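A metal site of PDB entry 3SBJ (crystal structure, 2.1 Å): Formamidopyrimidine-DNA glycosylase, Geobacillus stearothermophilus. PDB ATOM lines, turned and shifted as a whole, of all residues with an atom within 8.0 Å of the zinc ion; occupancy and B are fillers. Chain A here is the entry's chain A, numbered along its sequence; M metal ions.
SG of Cys 268 lies close to N of Arg 270, at 3.4 Å. The backbone NH of Cys 268 sits at hydrogen-bond distance from the side-chain amide oxygen of Gln 272, at 2.8 Å. The backbone NH (N) of Arg 250 sits close to the side-chain sulfur (SG) of Cys 248 (3.3 Å). N of Cys 248 is in hydrogen-bond range of O of Thr 253, at 2.7 Å. The side-chain sulfur (SG) of Cys 251 lies close to the side-chain hydroxyl (OG1) of Thr 253 (3.1 Å).
Within 4 Å of the zinc ion: Cys 248, Cys 251, Cys 268 and Cys 271. The nearest printed residue that does not touch the zinc ion is Phe 181 (4.04 Å).
The zinc ion is bound by SG of Cys 271. The side-chain sulfur (SG) of Cys 268 is bound to the zinc ion (2.4 Å). SG of Cys 248 binds the zinc ion. The zinc ion is bound by the side-chain sulfur (SG) of Cys 251 (2.4 Å).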
ATOM      1  N   PHE A 181      -8.129 -22.811  23.550  1.00  0.00           N
ATOM      2  CA  PHE A 181      -7.510 -21.971  22.539  1.00  0.00           C
ATOM      3  C   PHE A 181      -7.152 -20.596  23.105  1.00  0.00           C
ATOM      4  O   PHE A 181      -6.054 -20.082  22.882  1.00  0.00           O
ATOM      5  CB  PHE A 181      -8.385 -21.768  21.305  1.00  0.00           C
ATOM      6  CG  PHE A 181      -7.916 -20.648  20.425  1.00  0.00           C
ATOM      7  CD1 PHE A 181      -6.868 -20.842  19.527  1.00  0.00           C
ATOM      8  CD2 PHE A 181      -8.459 -19.377  20.547  1.00  0.00           C
ATOM      9  CE1 PHE A 181      -6.400 -19.800  18.744  1.00  0.00           C
ATOM     10  CE2 PHE A 181      -7.990 -18.335  19.764  1.00  0.00           C
ATOM     11  CZ  PHE A 181      -6.958 -18.542  18.863  1.00  0.00           C
ATOM     12  N   TYR A 239     -13.529 -19.183  17.972  1.00  0.00           N
ATOM     13  CA  TYR A 239     -12.154 -19.136  17.514  1.00  0.00           C
ATOM     14  C   TYR A 239     -11.724 -20.418  16.794  1.00  0.00           C
ATOM     15  O   TYR A 239     -11.023 -20.357  15.792  1.00  0.00           O
ATOM     16  CB  TYR A 239     -11.198 -18.852  18.679  1.00  0.00           C
ATOM     17  CG  TYR A 239     -11.237 -17.444  19.192  1.00  0.00           C
ATOM     18  CD1 TYR A 239     -11.892 -17.119  20.378  1.00  0.00           C
ATOM     19  CD2 TYR A 239     -10.607 -16.414  18.497  1.00  0.00           C
ATOM     20  CE1 TYR A 239     -11.918 -15.820  20.854  1.00  0.00           C
ATOM     21  CE2 TYR A 239     -10.626 -15.104  18.961  1.00  0.00           C
ATOM     22  CZ  TYR A 239     -11.288 -14.816  20.145  1.00  0.00           C
ATOM     23  OH  TYR A 239     -11.311 -13.533  20.616  1.00  0.00           O
ATOM     24  N   VAL A 240     -12.140 -21.564  17.310  1.00  0.00           N
ATOM     25  CA  VAL A 240     -11.683 -22.834  16.753  1.00  0.00           C
ATOM     26  C   VAL A 240     -12.773 -23.880  16.506  1.00  0.00           C
ATOM     27  O   VAL A 240     -12.659 -24.699  15.590  1.00  0.00           O
ATOM     28  CB  VAL A 240     -10.577 -23.471  17.610  1.00  0.00           C
ATOM     29  CG1 VAL A 240      -9.359 -22.553  17.674  1.00  0.00           C
ATOM     30  CG2 VAL A 240     -11.103 -23.784  19.017  1.00  0.00           C
ATOM     31  N   PRO A 247      -8.649 -20.171   8.474  1.00  0.00           N
ATOM     32  CA  PRO A 247      -7.543 -19.491   9.141  1.00  0.00           C
ATOM     33  C   PRO A 247      -7.878 -19.116  10.583  1.00  0.00           C
ATOM     34  O   PRO A 247      -8.963 -18.628  10.874  1.00  0.00           O
ATOM     35  CB  PRO A 247      -7.349 -18.219   8.301  1.00  0.00           C
ATOM     36  CG  PRO A 247      -8.650 -18.022   7.579  1.00  0.00           C
ATOM     37  CD  PRO A 247      -9.193 -19.398   7.342  1.00  0.00           C
ATOM     38  N   CYS A 248      -6.935 -19.381  11.473  1.00  0.00           N
ATOM     39  CA  CYS A 248      -7.080 -18.961  12.856  1.00  0.00           C
ATOM     40  C   CYS A 248      -7.279 -17.449  12.895  1.00  0.00           C
ATOM     41  O   CYS A 248      -6.615 -16.713  12.168  1.00  0.00           O
ATOM     42  CB  CYS A 248      -5.836 -19.336  13.657  1.00  0.00           C
ATOM     43  SG  CYS A 248      -5.762 -18.546  15.272  1.00  0.00           S
ATOM     44  N   LYS A 249      -8.196 -17.000  13.736  1.00  0.00           N
ATOM     45  CA  LYS A 249      -8.561 -15.583  13.805  1.00  0.00           C
ATOM     46  C   LYS A 249      -7.466 -14.739  14.445  1.00  0.00           C
ATOM     47  O   LYS A 249      -7.474 -13.514  14.318  1.00  0.00           O
ATOM     48  CB  LYS A 249      -9.872 -15.391  14.567  1.00  0.00           C
ATOM     49  CG  LYS A 249     -11.090 -15.955  13.836  1.00  0.00           C
ATOM     50  CD  LYS A 249     -12.374 -15.675  14.605  1.00  0.00           C
ATOM     51  CE  LYS A 249     -13.600 -16.118  13.828  1.00  0.00           C
ATOM     52  NZ  LYS A 249     -14.858 -15.895  14.595  1.00  0.00           N
ATOM     53  N   ARG A 250      -6.517 -15.377  15.114  1.00  0.00           N
ATOM     54  CA  ARG A 250      -5.443 -14.631  15.766  1.00  0.00           C
ATOM     55  C   ARG A 250      -4.081 -14.744  15.073  1.00  0.00           C
ATOM     56  O   ARG A 250      -3.218 -13.889  15.269  1.00  0.00           O
ATOM     57  CB  ARG A 250      -5.338 -14.994  17.246  1.00  0.00           C
ATOM     58  CG  ARG A 250      -6.482 -14.468  18.095  1.00  0.00           C
ATOM     59  CD  ARG A 250      -6.260 -14.761  19.565  1.00  0.00           C
ATOM     60  NE  ARG A 250      -7.368 -14.283  20.391  1.00  0.00           N
ATOM     61  CZ  ARG A 250      -7.568 -14.660  21.646  1.00  0.00           C
ATOM     62  NH1 ARG A 250      -6.749 -15.538  22.215  1.00  0.00           N
ATOM     63  NH2 ARG A 250      -8.597 -14.179  22.335  1.00  0.00           N
ATOM     64  N   CYS A 251      -3.873 -15.792  14.286  1.00  0.00           N
ATOM     65  CA  CYS A 251      -2.595 -15.947  13.588  1.00  0.00           C
ATOM     66  C   CYS A 251      -2.695 -16.401  12.126  1.00  0.00           C
ATOM     67  O   CYS A 251      -1.687 -16.398  11.409  1.00  0.00           O
ATOM     68  CB  CYS A 251      -1.690 -16.913  14.362  1.00  0.00           C
ATOM     69  SG  CYS A 251      -2.113 -18.629  14.083  1.00  0.00           S
ATOM     70  N   GLY A 252      -3.885 -16.807  11.708  1.00  0.00           N
ATOM     71  CA  GLY A 252      -4.111 -17.157  10.320  1.00  0.00           C
ATOM     72  C   GLY A 252      -3.712 -18.576   9.939  1.00  0.00           C
ATOM     73  O   GLY A 252      -3.975 -19.015   8.823  1.00  0.00           O
ATOM     74  N   THR A 253      -3.081 -19.284  10.870  1.00  0.00           N
ATOM     75  CA  THR A 253      -2.754 -20.691  10.659  1.00  0.00           C
ATOM     76  C   THR A 253      -4.047 -21.506  10.556  1.00  0.00           C
ATOM     77  O   THR A 253      -4.983 -21.302  11.331  1.00  0.00           O
ATOM     78  CB  THR A 253      -1.906 -21.246  11.814  1.00  0.00           C
ATOM     79  OG1 THR A 253      -0.719 -20.458  11.955  1.00  0.00           O
ATOM     80  CG2 THR A 253      -1.519 -22.694  11.567  1.00  0.00           C
ATOM     81  N   PRO A 254      -4.111 -22.435   9.585  1.00  0.00           N
ATOM     82  CA  PRO A 254      -5.361 -23.188   9.459  1.00  0.00           C
ATOM     83  C   PRO A 254      -5.688 -23.923  10.750  1.00  0.00           C
ATOM     84  O   PRO A 254      -4.830 -24.607  11.318  1.00  0.00           O
ATOM     85  CB  PRO A 254      -5.053 -24.187   8.340  1.00  0.00           C
ATOM     86  CG  PRO A 254      -3.969 -23.525   7.527  1.00  0.00           C
ATOM     87  CD  PRO A 254      -3.136 -22.769   8.521  1.00  0.00           C
ATOM     88  N   ILE A 255      -6.915 -23.763  11.225  1.00  0.00           N
ATOM     89  CA  ILE A 255      -7.371 -24.514  12.396  1.00  0.00           C
ATOM     90  C   ILE A 255      -7.380 -25.987  12.022  1.00  0.00           C
ATOM     91  O   ILE A 255      -7.759 -26.349  10.913  1.00  0.00           O
ATOM     92  CB  ILE A 255      -8.770 -24.061  12.832  1.00  0.00           C
ATOM     93  CG1 ILE A 255      -8.738 -22.592  13.254  1.00  0.00           C
ATOM     94  CG2 ILE A 255      -9.293 -24.939  13.965  1.00  0.00           C
ATOM     95  CD1 ILE A 255      -7.671 -22.316  14.314  1.00  0.00           C
ATOM     96  N   TYR A 267      -8.309 -26.956  17.296  1.00  0.00           N
ATOM     97  CA  TYR A 267      -7.231 -26.188  17.895  1.00  0.00           C
ATOM     98  C   TYR A 267      -6.382 -25.521  16.827  1.00  0.00           C
ATOM     99  O   TYR A 267      -6.408 -25.906  15.651  1.00  0.00           O
ATOM    100  CB  TYR A 267      -6.347 -27.091  18.753  1.00  0.00           C
ATOM    101  CG  TYR A 267      -5.625 -28.146  17.928  1.00  0.00           C
ATOM    102  CD1 TYR A 267      -4.326 -27.934  17.491  1.00  0.00           C
ATOM    103  CD2 TYR A 267      -6.255 -29.334  17.580  1.00  0.00           C
ATOM    104  CE1 TYR A 267      -3.673 -28.886  16.736  1.00  0.00           C
ATOM    105  CE2 TYR A 267      -5.610 -30.293  16.824  1.00  0.00           C
ATOM    106  CZ  TYR A 267      -4.317 -30.066  16.413  1.00  0.00           C
ATOM    107  OH  TYR A 267      -3.656 -31.011  15.660  1.00  0.00           O
ATOM    108  N   CYS A 268      -5.639 -24.509  17.237  1.00  0.00           N
ATOM    109  CA  CYS A 268      -4.657 -23.891  16.375  1.00  0.00           C
ATOM    110  C   CYS A 268      -3.290 -24.418  16.774  1.00  0.00           C
ATOM    111  O   CYS A 268      -2.875 -24.250  17.922  1.00  0.00           O
ATOM    112  CB  CYS A 268      -4.686 -22.371  16.500  1.00  0.00           C
ATOM    113  SG  CYS A 268      -3.353 -21.636  15.542  1.00  0.00           S
ATOM    114  N   PRO A 269      -2.590 -25.059  15.828  1.00  0.00           N
ATOM    115  CA  PRO A 269      -1.284 -25.661  16.116  1.00  0.00           C
ATOM    116  C   PRO A 269      -0.224 -24.607  16.404  1.00  0.00           C
ATOM    117  O   PRO A 269       0.862 -24.952  16.865  1.00  0.00           O
ATOM    118  CB  PRO A 269      -0.954 -26.396  14.810  1.00  0.00           C
ATOM    119  CG  PRO A 269      -1.722 -25.682  13.759  1.00  0.00           C
ATOM    120  CD  PRO A 269      -2.994 -25.233  14.428  1.00  0.00           C
ATOM    121  N   ARG A 270      -0.527 -23.348  16.124  1.00  0.00           N
ATOM    122  CA  ARG A 270       0.436 -22.279  16.415  1.00  0.00           C
ATOM    123  C   ARG A 270       0.149 -21.580  17.744  1.00  0.00           C
ATOM    124  O   ARG A 270       1.041 -21.441  18.573  1.00  0.00           O
ATOM    125  CB  ARG A 270       0.506 -21.259  15.280  1.00  0.00           C
ATOM    126  CG  ARG A 270       1.541 -20.184  15.524  1.00  0.00           C
ATOM    127  CD  ARG A 270       1.619 -19.195  14.356  1.00  0.00           C
ATOM    128  NE  ARG A 270       2.674 -18.213  14.596  1.00  0.00           N
ATOM    129  CZ  ARG A 270       3.075 -17.312  13.698  1.00  0.00           C
ATOM    130  NH1 ARG A 270       4.050 -16.468  14.016  1.00  0.00           N
ATOM    131  NH2 ARG A 270       2.507 -17.265  12.501  1.00  0.00           N
ATOM    132  N   CYS A 271      -1.090 -21.128  17.933  1.00  0.00           N
ATOM    133  CA  CYS A 271      -1.459 -20.424  19.159  1.00  0.00           C
ATOM    134  C   CYS A 271      -1.437 -21.339  20.376  1.00  0.00           C
ATOM    135  O   CYS A 271      -1.207 -20.894  21.496  1.00  0.00           O
ATOM    136  CB  CYS A 271      -2.845 -19.787  19.042  1.00  0.00           C
ATOM    137  SG  CYS A 271      -2.947 -18.429  17.863  1.00  0.00           S
ATOM    138  N   GLN A 272      -1.691 -22.629  20.165  1.00  0.00           N
ATOM    139  CA  GLN A 272      -1.791 -23.544  21.296  1.00  0.00           C
ATOM    140  C   GLN A 272      -0.548 -24.419  21.446  1.00  0.00           C
ATOM    141  O   GLN A 272      -0.042 -24.964  20.460  1.00  0.00           O
ATOM    142  CB  GLN A 272      -3.059 -24.385  21.191  1.00  0.00           C
ATOM    143  CG  GLN A 272      -4.318 -23.555  21.426  1.00  0.00           C
ATOM    144  CD  GLN A 272      -5.587 -24.290  21.012  1.00  0.00           C
ATOM    145  OE1 GLN A 272      -6.106 -24.065  19.919  1.00  0.00           O
ATOM    146  NE2 GLN A 272      -6.091 -25.149  21.877  1.00  0.00           N
HETATM  147 ZN    ZN M   1      -3.601 -19.320  15.864  1.00  0.00          ZN
